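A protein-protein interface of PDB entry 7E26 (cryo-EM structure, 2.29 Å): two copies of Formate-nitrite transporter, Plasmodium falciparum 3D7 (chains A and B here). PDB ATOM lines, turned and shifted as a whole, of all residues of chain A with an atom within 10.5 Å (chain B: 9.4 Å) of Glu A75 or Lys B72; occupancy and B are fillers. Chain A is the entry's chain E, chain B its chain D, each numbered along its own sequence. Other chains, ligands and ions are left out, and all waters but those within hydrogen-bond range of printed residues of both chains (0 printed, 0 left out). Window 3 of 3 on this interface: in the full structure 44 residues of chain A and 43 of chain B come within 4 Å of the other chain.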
ATOM      1  N   PHE A  68     -20.600  17.471  -7.870  1.00  0.00           N
ATOM      2  CA  PHE A  68     -19.922  18.432  -8.727  1.00  0.00           C
ATOM      3  C   PHE A  68     -20.816  19.589  -9.140  1.00  0.00           C
ATOM      4  O   PHE A  68     -20.399  20.415  -9.955  1.00  0.00           O
ATOM      5  CB  PHE A  68     -19.371  17.724  -9.965  1.00  0.00           C
ATOM      6  CG  PHE A  68     -18.115  16.955  -9.700  1.00  0.00           C
ATOM      7  CD1 PHE A  68     -18.168  15.680  -9.160  1.00  0.00           C
ATOM      8  CD2 PHE A  68     -16.880  17.513  -9.961  1.00  0.00           C
ATOM      9  CE1 PHE A  68     -17.015  14.977  -8.897  1.00  0.00           C
ATOM     10  CE2 PHE A  68     -15.724  16.814  -9.702  1.00  0.00           C
ATOM     11  CZ  PHE A  68     -15.793  15.544  -9.171  1.00  0.00           C
ATOM     12  N   TYR A  69     -22.028  19.662  -8.603  1.00  0.00           N
ATOM     13  CA  TYR A  69     -22.952  20.753  -8.854  1.00  0.00           C
ATOM     14  C   TYR A  69     -22.946  21.743  -7.698  1.00  0.00           C
ATOM     15  O   TYR A  69     -23.940  22.442  -7.475  1.00  0.00           O
ATOM     16  CB  TYR A  69     -24.345  20.174  -9.100  1.00  0.00           C
ATOM     17  CG  TYR A  69     -25.309  21.040  -9.867  1.00  0.00           C
ATOM     18  CD1 TYR A  69     -25.123  21.270 -11.225  1.00  0.00           C
ATOM     19  CD2 TYR A  69     -26.441  21.560  -9.265  1.00  0.00           C
ATOM     20  CE1 TYR A  69     -26.006  22.034 -11.942  1.00  0.00           C
ATOM     21  CE2 TYR A  69     -27.331  22.321  -9.978  1.00  0.00           C
ATOM     22  CZ  TYR A  69     -27.110  22.553 -11.314  1.00  0.00           C
ATOM     23  OH  TYR A  69     -27.991  23.309 -12.032  1.00  0.00           O
ATOM     24  N   TYR A  70     -21.848  21.777  -6.943  1.00  0.00           N
ATOM     25  CA  TYR A  70     -21.680  22.691  -5.824  1.00  0.00           C
ATOM     26  C   TYR A  70     -21.717  24.128  -6.319  1.00  0.00           C
ATOM     27  O   TYR A  70     -21.223  24.431  -7.404  1.00  0.00           O
ATOM     28  CB  TYR A  70     -20.354  22.379  -5.132  1.00  0.00           C
ATOM     29  CG  TYR A  70     -20.022  23.200  -3.911  1.00  0.00           C
ATOM     30  CD1 TYR A  70     -20.646  22.962  -2.699  1.00  0.00           C
ATOM     31  CD2 TYR A  70     -19.055  24.191  -3.966  1.00  0.00           C
ATOM     32  CE1 TYR A  70     -20.330  23.704  -1.582  1.00  0.00           C
ATOM     33  CE2 TYR A  70     -18.734  24.934  -2.858  1.00  0.00           C
ATOM     34  CZ  TYR A  70     -19.372  24.689  -1.670  1.00  0.00           C
ATOM     35  OH  TYR A  70     -19.049  25.435  -0.567  1.00  0.00           O
ATOM     36  N   HIS A  71     -22.313  25.016  -5.518  1.00  0.00           N
ATOM     37  CA  HIS A  71     -22.724  26.326  -6.013  1.00  0.00           C
ATOM     38  C   HIS A  71     -21.560  27.253  -6.336  1.00  0.00           C
ATOM     39  O   HIS A  71     -21.744  28.203  -7.100  1.00  0.00           O
ATOM     40  CB  HIS A  71     -23.659  26.990  -5.002  1.00  0.00           C
ATOM     41  CG  HIS A  71     -22.979  27.471  -3.762  1.00  0.00           C
ATOM     42  ND1 HIS A  71     -23.027  28.785  -3.352  1.00  0.00           N
ATOM     43  CD2 HIS A  71     -22.241  26.816  -2.837  1.00  0.00           C
ATOM     44  CE1 HIS A  71     -22.348  28.917  -2.227  1.00  0.00           C
ATOM     45  NE2 HIS A  71     -21.859  27.737  -1.896  1.00  0.00           N
ATOM     46  N   LYS A  72     -20.374  27.002  -5.792  1.00  0.00           N
ATOM     47  CA  LYS A  72     -19.198  27.773  -6.164  1.00  0.00           C
ATOM     48  C   LYS A  72     -18.500  27.203  -7.387  1.00  0.00           C
ATOM     49  O   LYS A  72     -17.897  27.958  -8.155  1.00  0.00           O
ATOM     50  CB  LYS A  72     -18.218  27.836  -4.994  1.00  0.00           C
ATOM     51  CG  LYS A  72     -18.689  28.686  -3.844  1.00  0.00           C
ATOM     52  CD  LYS A  72     -18.946  30.100  -4.294  1.00  0.00           C
ATOM     53  CE  LYS A  72     -19.214  31.005  -3.119  1.00  0.00           C
ATOM     54  NZ  LYS A  72     -19.620  32.361  -3.565  1.00  0.00           N
ATOM     55  N   LEU A  73     -18.562  25.886  -7.576  1.00  0.00           N
ATOM     56  CA  LEU A  73     -18.057  25.264  -8.791  1.00  0.00           C
ATOM     57  C   LEU A  73     -19.005  25.480  -9.961  1.00  0.00           C
ATOM     58  O   LEU A  73     -18.558  25.608 -11.104  1.00  0.00           O
ATOM     59  CB  LEU A  73     -17.839  23.772  -8.545  1.00  0.00           C
ATOM     60  CG  LEU A  73     -17.304  22.891  -9.668  1.00  0.00           C
ATOM     61  CD1 LEU A  73     -15.929  23.344 -10.098  1.00  0.00           C
ATOM     62  CD2 LEU A  73     -17.275  21.455  -9.216  1.00  0.00           C
ATOM     63  N   ARG A  74     -20.308  25.543  -9.682  1.00  0.00           N
ATOM     64  CA  ARG A  74     -21.326  25.774 -10.701  1.00  0.00           C
ATOM     65  C   ARG A  74     -21.209  27.159 -11.327  1.00  0.00           C
ATOM     66  O   ARG A  74     -21.640  27.359 -12.466  1.00  0.00           O
ATOM     67  CB  ARG A  74     -22.702  25.590 -10.069  1.00  0.00           C
ATOM     68  CG  ARG A  74     -23.824  25.243 -10.992  1.00  0.00           C
ATOM     69  CD  ARG A  74     -25.135  25.552 -10.310  1.00  0.00           C
ATOM     70  NE  ARG A  74     -25.237  24.885  -9.018  1.00  0.00           N
ATOM     71  CZ  ARG A  74     -26.101  25.219  -8.067  1.00  0.00           C
ATOM     72  NH1 ARG A  74     -26.126  24.546  -6.927  1.00  0.00           N
ATOM     73  NH2 ARG A  74     -26.940  26.222  -8.255  1.00  0.00           N
ATOM     74  N   GLU A  75     -20.641  28.126 -10.604  1.00  0.00           N
ATOM     75  CA  GLU A  75     -20.478  29.470 -11.140  1.00  0.00           C
ATOM     76  C   GLU A  75     -19.373  29.558 -12.181  1.00  0.00           C
ATOM     77  O   GLU A  75     -19.371  30.494 -12.983  1.00  0.00           O
ATOM     78  CB  GLU A  75     -20.175  30.453 -10.015  1.00  0.00           C
ATOM     79  CG  GLU A  75     -21.363  30.828  -9.176  1.00  0.00           C
ATOM     80  CD  GLU A  75     -20.964  31.587  -7.934  1.00  0.00           C
ATOM     81  OE1 GLU A  75     -19.866  32.178  -7.931  1.00  0.00           O
ATOM     82  OE2 GLU A  75     -21.742  31.587  -6.958  1.00  0.00           O
ATOM     83  N   ILE A  76     -18.436  28.620 -12.180  1.00  0.00           N
ATOM     84  CA  ILE A  76     -17.303  28.642 -13.091  1.00  0.00           C
ATOM     85  C   ILE A  76     -17.523  27.720 -14.276  1.00  0.00           C
ATOM     86  O   ILE A  76     -17.367  28.127 -15.425  1.00  0.00           O
ATOM     87  CB  ILE A  76     -16.006  28.277 -12.336  1.00  0.00           C
ATOM     88  CG1 ILE A  76     -15.827  29.175 -11.116  1.00  0.00           C
ATOM     89  CG2 ILE A  76     -14.809  28.381 -13.259  1.00  0.00           C
ATOM     90  CD1 ILE A  76     -14.815  28.658 -10.138  1.00  0.00           C
ATOM     91  N   VAL A  77     -17.891  26.465 -14.021  1.00  0.00           N
ATOM     92  CA  VAL A  77     -17.984  25.474 -15.086  1.00  0.00           C
ATOM     93  C   VAL A  77     -19.412  25.206 -15.529  1.00  0.00           C
ATOM     94  O   VAL A  77     -19.611  24.473 -16.510  1.00  0.00           O
ATOM     95  CB  VAL A  77     -17.314  24.148 -14.675  1.00  0.00           C
ATOM     96  CG1 VAL A  77     -15.900  24.398 -14.197  1.00  0.00           C
ATOM     97  CG2 VAL A  77     -18.124  23.453 -13.606  1.00  0.00           C
ATOM     98  N   GLY A  78     -20.406  25.781 -14.860  1.00  0.00           N
ATOM     99  CA  GLY A  78     -21.781  25.490 -15.219  1.00  0.00           C
ATOM    100  C   GLY A  78     -22.171  24.095 -14.774  1.00  0.00           C
ATOM    101  O   GLY A  78     -21.893  23.673 -13.650  1.00  0.00           O
ATOM    102  N   ALA A  79     -22.814  23.360 -15.674  1.00  0.00           N
ATOM    103  CA  ALA A  79     -23.236  21.996 -15.405  1.00  0.00           C
ATOM    104  C   ALA A  79     -22.394  20.967 -16.140  1.00  0.00           C
ATOM    105  O   ALA A  79     -22.855  19.848 -16.350  1.00  0.00           O
ATOM    106  CB  ALA A  79     -24.708  21.818 -15.769  1.00  0.00           C
ATOM    107  N   SER A  80     -21.166  21.314 -16.521  1.00  0.00           N
ATOM    108  CA  SER A  80     -20.378  20.440 -17.385  1.00  0.00           C
ATOM    109  C   SER A  80     -19.836  19.236 -16.625  1.00  0.00           C
ATOM    110  O   SER A  80     -20.009  18.087 -17.054  1.00  0.00           O
ATOM    111  CB  SER A  80     -19.241  21.236 -18.015  1.00  0.00           C
ATOM    112  OG  SER A  80     -18.505  21.934 -17.034  1.00  0.00           O
ATOM    113  N   MET A  81     -19.178  19.480 -15.493  1.00  0.00           N
ATOM    114  CA  MET A  81     -18.603  18.408 -14.696  1.00  0.00           C
ATOM    115  C   MET A  81     -19.661  17.533 -14.040  1.00  0.00           C
ATOM    116  O   MET A  81     -19.420  16.338 -13.857  1.00  0.00           O
ATOM    117  CB  MET A  81     -17.667  18.993 -13.641  1.00  0.00           C
ATOM    118  CG  MET A  81     -16.423  19.630 -14.232  1.00  0.00           C
ATOM    119  SD  MET A  81     -15.432  20.549 -13.047  1.00  0.00           S
ATOM    120  CE  MET A  81     -14.431  19.246 -12.350  1.00  0.00           C
ATOM    121  N   SER A  82     -20.835  18.091 -13.734  1.00  0.00           N
ATOM    122  CA  SER A  82     -21.942  17.298 -13.211  1.00  0.00           C
ATOM    123  C   SER A  82     -22.424  16.268 -14.222  1.00  0.00           C
ATOM    124  O   SER A  82     -22.588  15.090 -13.886  1.00  0.00           O
ATOM    125  CB  SER A  82     -23.092  18.217 -12.826  1.00  0.00           C
ATOM    126  OG  SER A  82     -22.713  19.096 -11.797  1.00  0.00           O
ATOM    127  N   VAL A 161     -28.152  27.036   0.069  1.00  0.00           N
ATOM    128  CA  VAL A 161     -27.520  26.941  -1.245  1.00  0.00           C
ATOM    129  C   VAL A 161     -26.170  26.229  -1.195  1.00  0.00           C
ATOM    130  O   VAL A 161     -25.760  25.618  -2.188  1.00  0.00           O
ATOM    131  CB  VAL A 161     -27.428  28.355  -1.863  1.00  0.00           C
ATOM    132  CG1 VAL A 161     -26.393  29.219  -1.158  1.00  0.00           C
ATOM    133  CG2 VAL A 161     -27.165  28.300  -3.362  1.00  0.00           C
ATOM    134  N   GLU A 162     -25.495  26.225  -0.047  1.00  0.00           N
ATOM    135  CA  GLU A 162     -24.240  25.500   0.083  1.00  0.00           C
ATOM    136  C   GLU A 162     -24.441  24.014   0.337  1.00  0.00           C
ATOM    137  O   GLU A 162     -23.469  23.256   0.269  1.00  0.00           O
ATOM    138  CB  GLU A 162     -23.395  26.105   1.204  1.00  0.00           C
ATOM    139  CG  GLU A 162     -23.979  25.942   2.589  1.00  0.00           C
ATOM    140  CD  GLU A 162     -24.852  27.108   2.993  1.00  0.00           C
ATOM    141  OE1 GLU A 162     -24.955  28.071   2.207  1.00  0.00           O
ATOM    142  OE2 GLU A 162     -25.436  27.062   4.093  1.00  0.00           O
ATOM    143  N   HIS A 165     -27.166  21.065  -3.270  1.00  0.00           N
ATOM    144  CA  HIS A 165     -26.696  20.799  -4.623  1.00  0.00           C
ATOM    145  C   HIS A 165     -27.055  19.413  -5.143  1.00  0.00           C
ATOM    146  O   HIS A 165     -26.767  19.122  -6.305  1.00  0.00           O
ATOM    147  CB  HIS A 165     -25.186  21.045  -4.698  1.00  0.00           C
ATOM    148  CG  HIS A 165     -24.411  20.436  -3.575  1.00  0.00           C
ATOM    149  ND1 HIS A 165     -23.905  19.158  -3.620  1.00  0.00           N
ATOM    150  CD2 HIS A 165     -24.050  20.941  -2.373  1.00  0.00           C
ATOM    151  CE1 HIS A 165     -23.272  18.898  -2.491  1.00  0.00           C
ATOM    152  NE2 HIS A 165     -23.347  19.965  -1.717  1.00  0.00           N
ATOM    153  N   LEU B  67     -20.963  21.723 -23.378  1.00  0.00           N
ATOM    154  CA  LEU B  67     -21.104  21.829 -21.929  1.00  0.00           C
ATOM    155  C   LEU B  67     -19.885  22.484 -21.301  1.00  0.00           C
ATOM    156  O   LEU B  67     -20.019  23.351 -20.432  1.00  0.00           O
ATOM    157  CB  LEU B  67     -21.330  20.454 -21.315  1.00  0.00           C
ATOM    158  CG  LEU B  67     -22.775  20.007 -21.130  1.00  0.00           C
ATOM    159  CD1 LEU B  67     -22.792  18.538 -20.825  1.00  0.00           C
ATOM    160  CD2 LEU B  67     -23.441  20.796 -20.033  1.00  0.00           C
ATOM    161  N   PHE B  68     -18.692  22.092 -21.733  1.00  0.00           N
ATOM    162  CA  PHE B  68     -17.448  22.639 -21.213  1.00  0.00           C
ATOM    163  C   PHE B  68     -17.042  23.935 -21.895  1.00  0.00           C
ATOM    164  O   PHE B  68     -15.953  24.445 -21.626  1.00  0.00           O
ATOM    165  CB  PHE B  68     -16.332  21.604 -21.341  1.00  0.00           C
ATOM    166  CG  PHE B  68     -16.391  20.533 -20.296  1.00  0.00           C
ATOM    167  CD1 PHE B  68     -17.235  19.447 -20.446  1.00  0.00           C
ATOM    168  CD2 PHE B  68     -15.626  20.628 -19.151  1.00  0.00           C
ATOM    169  CE1 PHE B  68     -17.305  18.470 -19.478  1.00  0.00           C
ATOM    170  CE2 PHE B  68     -15.692  19.654 -18.181  1.00  0.00           C
ATOM    171  CZ  PHE B  68     -16.531  18.574 -18.347  1.00  0.00           C
ATOM    172  N   TYR B  69     -17.887  24.470 -22.769  1.00  0.00           N
ATOM    173  CA  TYR B  69     -17.656  25.739 -23.434  1.00  0.00           C
ATOM    174  C   TYR B  69     -18.452  26.852 -22.769  1.00  0.00           C
ATOM    175  O   TYR B  69     -18.778  27.853 -23.415  1.00  0.00           O
ATOM    176  CB  TYR B  69     -18.010  25.592 -24.915  1.00  0.00           C
ATOM    177  CG  TYR B  69     -17.376  26.580 -25.860  1.00  0.00           C
ATOM    178  CD1 TYR B  69     -16.016  26.516 -26.140  1.00  0.00           C
ATOM    179  CD2 TYR B  69     -18.139  27.518 -26.532  1.00  0.00           C
ATOM    180  CE1 TYR B  69     -15.431  27.391 -27.018  1.00  0.00           C
ATOM    181  CE2 TYR B  69     -17.560  28.393 -27.415  1.00  0.00           C
ATOM    182  CZ  TYR B  69     -16.210  28.323 -27.655  1.00  0.00           C
ATOM    183  OH  TYR B  69     -15.625  29.190 -28.534  1.00  0.00           O
ATOM    184  N   TYR B  70     -18.797  26.662 -21.495  1.00  0.00           N
ATOM    185  CA  TYR B  70     -19.530  27.648 -20.716  1.00  0.00           C
ATOM    186  C   TYR B  70     -18.712  28.924 -20.592  1.00  0.00           C
ATOM    187  O   TYR B  70     -17.488  28.876 -20.477  1.00  0.00           O
ATOM    188  CB  TYR B  70     -19.838  27.054 -19.342  1.00  0.00           C
ATOM    189  CG  TYR B  70     -20.638  27.917 -18.400  1.00  0.00           C
ATOM    190  CD1 TYR B  70     -22.001  28.087 -18.567  1.00  0.00           C
ATOM    191  CD2 TYR B  70     -20.032  28.532 -17.316  1.00  0.00           C
ATOM    192  CE1 TYR B  70     -22.731  28.864 -17.698  1.00  0.00           C
ATOM    193  CE2 TYR B  70     -20.753  29.308 -16.442  1.00  0.00           C
ATOM    194  CZ  TYR B  70     -22.100  29.472 -16.637  1.00  0.00           C
ATOM    195  OH  TYR B  70     -22.815  30.249 -15.761  1.00  0.00           O
ATOM    196  N   HIS B  71     -19.396  30.071 -20.623  1.00  0.00           N
ATOM    197  CA  HIS B  71     -18.727  31.345 -20.865  1.00  0.00           C
ATOM    198  C   HIS B  71     -17.831  31.795 -19.719  1.00  0.00           C
ATOM    199  O   HIS B  71     -16.939  32.618 -19.941  1.00  0.00           O
ATOM    200  CB  HIS B  71     -19.764  32.423 -21.176  1.00  0.00           C
ATOM    201  CG  HIS B  71     -20.564  32.862 -19.993  1.00  0.00           C
ATOM    202  ND1 HIS B  71     -20.611  34.173 -19.574  1.00  0.00           N
ATOM    203  CD2 HIS B  71     -21.356  32.169 -19.143  1.00  0.00           C
ATOM    204  CE1 HIS B  71     -21.397  34.268 -18.517  1.00  0.00           C
ATOM    205  NE2 HIS B  71     -21.859  33.065 -18.235  1.00  0.00           N
ATOM    206  N   LYS B  72     -18.031  31.279 -18.512  1.00  0.00           N
ATOM    207  CA  LYS B  72     -17.127  31.572 -17.410  1.00  0.00           C
ATOM    208  C   LYS B  72     -15.943  30.620 -17.368  1.00  0.00           C
ATOM    209  O   LYS B  72     -14.858  31.014 -16.931  1.00  0.00           O
ATOM    210  CB  LYS B  72     -17.880  31.514 -16.081  1.00  0.00           C
ATOM    211  CG  LYS B  72     -18.855  32.644 -15.880  1.00  0.00           C
ATOM    212  CD  LYS B  72     -18.152  33.975 -15.943  1.00  0.00           C
ATOM    213  CE  LYS B  72     -19.072  35.097 -15.536  1.00  0.00           C
ATOM    214  NZ  LYS B  72     -18.434  36.420 -15.747  1.00  0.00           N
ATOM    215  N   LEU B  73     -16.133  29.378 -17.804  1.00  0.00           N
ATOM    216  CA  LEU B  73     -15.030  28.440 -17.947  1.00  0.00           C
ATOM    217  C   LEU B  73     -14.194  28.748 -19.179  1.00  0.00           C
ATOM    218  O   LEU B  73     -12.977  28.542 -19.168  1.00  0.00           O
ATOM    219  CB  LEU B  73     -15.578  27.014 -18.011  1.00  0.00           C
ATOM    220  CG  LEU B  73     -14.617  25.840 -18.153  1.00  0.00           C
ATOM    221  CD1 LEU B  73     -13.683  25.765 -16.969  1.00  0.00           C
ATOM    222  CD2 LEU B  73     -15.397  24.562 -18.300  1.00  0.00           C
ATOM    223  N   ARG B  74     -14.833  29.259 -20.232  1.00  0.00           N
ATOM    224  CA  ARG B  74     -14.151  29.628 -21.468  1.00  0.00           C
ATOM    225  C   ARG B  74     -13.181  30.786 -21.268  1.00  0.00           C
ATOM    226  O   ARG B  74     -12.218  30.922 -22.028  1.00  0.00           O
ATOM    227  CB  ARG B  74     -15.201  29.990 -22.517  1.00  0.00           C
ATOM    228  CG  ARG B  74     -14.792  29.865 -23.947  1.00  0.00           C
ATOM    229  CD  ARG B  74     -15.737  30.676 -24.800  1.00  0.00           C
ATOM    230  NE  ARG B  74     -17.125  30.293 -24.574  1.00  0.00           N
ATOM    231  CZ  ARG B  74     -18.173  31.031 -24.921  1.00  0.00           C
ATOM    232  NH1 ARG B  74     -19.400  30.595 -24.682  1.00  0.00           N
ATOM    233  NH2 ARG B  74     -17.996  32.202 -25.507  1.00  0.00           N
ATOM    234  N   GLU B  75     -13.416  31.631 -20.262  1.00  0.00           N
ATOM    235  CA  GLU B  75     -12.522  32.751 -19.995  1.00  0.00           C
ATOM    236  C   GLU B  75     -11.208  32.318 -19.367  1.00  0.00           C
ATOM    237  O   GLU B  75     -10.228  33.062 -19.439  1.00  0.00           O
ATOM    238  CB  GLU B  75     -13.201  33.759 -19.076  1.00  0.00           C
ATOM    239  CG  GLU B  75     -14.236  34.617 -19.746  1.00  0.00           C
ATOM    240  CD  GLU B  75     -15.051  35.405 -18.749  1.00  0.00           C
ATOM    241  OE1 GLU B  75     -14.562  35.615 -17.621  1.00  0.00           O
ATOM    242  OE2 GLU B  75     -16.183  35.807 -19.088  1.00  0.00           O
ATOM    243  N   ILE B  76     -11.166  31.147 -18.745  1.00  0.00           N
ATOM    244  CA  ILE B  76      -9.980  30.665 -18.058  1.00  0.00           C
ATOM    245  C   ILE B  76      -9.204  29.678 -18.911  1.00  0.00           C
ATOM    246  O   ILE B  76      -7.998  29.823 -19.097  1.00  0.00           O
ATOM    247  CB  ILE B  76     -10.367  30.041 -16.699  1.00  0.00           C
ATOM    248  CG1 ILE B  76     -11.193  31.024 -15.876  1.00  0.00           C
ATOM    249  CG2 ILE B  76      -9.129  29.613 -15.939  1.00  0.00           C
ATOM    250  CD1 ILE B  76     -11.914  30.382 -14.728  1.00  0.00           C
ATOM    251  N   VAL B  77      -9.878  28.660 -19.444  1.00  0.00           N
ATOM    252  CA  VAL B  77      -9.192  27.589 -20.155  1.00  0.00           C
ATOM    253  C   VAL B  77      -9.295  27.712 -21.665  1.00  0.00           C
ATOM    254  O   VAL B  77      -8.652  26.929 -22.379  1.00  0.00           O
ATOM    255  CB  VAL B  77      -9.710  26.205 -19.713  1.00  0.00           C
ATOM    256  CG1 VAL B  77      -9.648  26.075 -18.207  1.00  0.00           C
ATOM    257  CG2 VAL B  77     -11.118  25.982 -20.211  1.00  0.00           C
ATOM    258  N   GLY B  78     -10.062  28.670 -22.177  1.00  0.00           N
ATOM    259  CA  GLY B  78     -10.231  28.769 -23.613  1.00  0.00           C
ATOM    260  C   GLY B  78     -11.123  27.659 -24.128  1.00  0.00           C
ATOM    261  O   GLY B  78     -12.177  27.360 -23.563  1.00  0.00           O
ATOM    262  N   MET B  81     -10.754  22.287 -22.794  1.00  0.00           N
ATOM    263  CA  MET B  81     -11.589  21.233 -22.236  1.00  0.00           C
ATOM    264  C   MET B  81     -12.743  20.852 -23.151  1.00  0.00           C
ATOM    265  O   MET B  81     -13.148  19.689 -23.150  1.00  0.00           O
ATOM    266  CB  MET B  81     -12.114  21.660 -20.867  1.00  0.00           C
ATOM    267  CG  MET B  81     -11.025  21.770 -19.817  1.00  0.00           C
ATOM    268  SD  MET B  81     -11.564  22.514 -18.271  1.00  0.00           S
ATOM    269  CE  MET B  81     -12.234  21.095 -17.422  1.00  0.00           C
ATOM    270  N   VAL B 161     -25.771  34.698 -23.332  1.00  0.00           N
ATOM    271  CA  VAL B 161     -24.401  34.197 -23.272  1.00  0.00           C
ATOM    272  C   VAL B 161     -24.218  33.116 -22.207  1.00  0.00           C
ATOM    273  O   VAL B 161     -23.343  32.254 -22.349  1.00  0.00           O
ATOM    274  CB  VAL B 161     -23.436  35.391 -23.082  1.00  0.00           C
ATOM    275  CG1 VAL B 161     -23.538  35.989 -21.687  1.00  0.00           C
ATOM    276  CG2 VAL B 161     -21.998  35.014 -23.412  1.00  0.00           C
ATOM    277  N   GLU B 162     -25.063  33.088 -21.177  1.00  0.00           N
ATOM    278  CA  GLU B 162     -24.986  32.038 -20.174  1.00  0.00           C
ATOM    279  C   GLU B 162     -25.669  30.752 -20.611  1.00  0.00           C
ATOM    280  O   GLU B 162     -25.506  29.728 -19.941  1.00  0.00           O
ATOM    281  CB  GLU B 162     -25.593  32.523 -18.857  1.00  0.00           C
ATOM    282  CG  GLU B 162     -27.083  32.778 -18.909  1.00  0.00           C
ATOM    283  CD  GLU B 162     -27.414  34.208 -19.269  1.00  0.00           C
ATOM    284  OE1 GLU B 162     -26.476  35.013 -19.423  1.00  0.00           O
ATOM    285  OE2 GLU B 162     -28.613  34.528 -19.398  1.00  0.00           O
ATOM    286  N   LYS B 163     -26.422  30.774 -21.712  1.00  0.00           N
ATOM    287  CA  LYS B 163     -27.112  29.596 -22.209  1.00  0.00           C
ATOM    288  C   LYS B 163     -26.718  29.191 -23.619  1.00  0.00           C
ATOM    289  O   LYS B 163     -27.075  28.086 -24.040  1.00  0.00           O
ATOM    290  CB  LYS B 163     -28.633  29.811 -22.176  1.00  0.00           C
ATOM    291  CG  LYS B 163     -29.160  30.374 -20.884  1.00  0.00           C
ATOM    292  CD  LYS B 163     -30.607  30.004 -20.676  1.00  0.00           C
ATOM    293  CE  LYS B 163     -31.298  31.001 -19.769  1.00  0.00           C
ATOM    294  NZ  LYS B 163     -31.678  32.239 -20.500  1.00  0.00           N
ATOM    295  N   HIS B 165     -23.976  28.258 -25.089  1.00  0.00           N
ATOM    296  CA  HIS B 165     -22.664  27.642 -25.227  1.00  0.00           C
ATOM    297  C   HIS B 165     -22.661  26.372 -26.070  1.00  0.00           C
ATOM    298  O   HIS B 165     -21.585  25.820 -26.309  1.00  0.00           O
ATOM    299  CB  HIS B 165     -22.067  27.387 -23.840  1.00  0.00           C
ATOM    300  CG  HIS B 165     -23.017  26.758 -22.872  1.00  0.00           C
ATOM    301  ND1 HIS B 165     -23.154  25.396 -22.736  1.00  0.00           N
ATOM    302  CD2 HIS B 165     -23.874  27.313 -21.986  1.00  0.00           C
ATOM    303  CE1 HIS B 165     -24.060  25.139 -21.812  1.00  0.00           C
ATOM    304  NE2 HIS B 165     -24.513  26.286 -21.343  1.00  0.00           N
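N of Leu B73 is in hydrogen-bond range of O of Ile A76 (3.0 Å).
The backbone carbonyl oxygen (O) of Val A77 sits at hydrogen-bond distance from the side-chain hydroxyl (OG) of Ser A80.
Glu A75 touches Tyr B70 (O to CE2, 3.9 Å). O of Glu A75 touches CB of Lys B72, 3.6 Å away. Ile A76 touches Tyr B70 (O to CD2, 3.3 Å). Ile A76 touches Lys B72. Ile B76 touches Ile A76. CG1 of Val A77 touches CD1 of Leu B73, at 3.8 Å. Leu B67 touches Ala A79. Ser A80 touches Leu B67. Phe B68 touches Ser A80. CZ of Phe B68 touches N of Met A81, at 3.997 Å.
Of chain B, only Tyr B70 (3.3 Å), Lys B72 (3.5 Å), Leu B73 (3.0 Å) and Ile B76 (3.8 Å) come within 4 Å of Ile A76. Tyr B70 touches just these residues of chain A: Glu A75 (3.9 Å), Ile A76 (3.3 Å), Val A77 (3.8 Å) and Gly A78 (3.7 Å). No residue of chain A comes within 4 Å of His B71. Leu B73 touches two residues of chain A. No residue of chain A comes within 4 Å of Glu B75. Of the printed residues of chain B, Gly A78 touches Tyr B70. Printed residues of chain A within 4 Å of Phe B68: Ser A80 and Met A81. Printed residues of chain B within 4 Å of Val A77: Tyr B70 and Leu B73. Of the printed residues of chain B, Ala A79 touches Leu B67. Arg B74 touches none of the printed residues of chain A.
Hydrophobic or aromatic side chains of chain A within 4 Å of the printed part of chain B: Ile A76 and Val A77. Hydrophobic or aromatic side chains of chain B that line the printed part of chain A: Leu B67, Phe B68, Tyr B70, Leu B73 and Ile B76. Along chain B the printed residues that touch a printed residue of chain A span positions 67 to 76. Among the printed residues, 13 pairs touch across the chains. Among the printed residues, no Asp or Glu carboxylate lies within 4 Å of a Lys or Arg side-chain nitrogen of the other chain.
Glu A75 touches Tyr B70, but with the chains exchanged Tyr A70 does not touch Glu B75 (16.5 Å). Ile A76 touches Leu B73, but with the chains exchanged Leu A73 does not touch Ile B76 (8.9 Å). Val A77 touches Tyr B70, but with the chains exchanged Tyr A70 does not touch Val B77 (15.9 Å). Val A77 touches Leu B73, but with the chains exchanged Leu A73 does not touch Val B77 (10.6 Å). 15 positions are printed for both chains.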
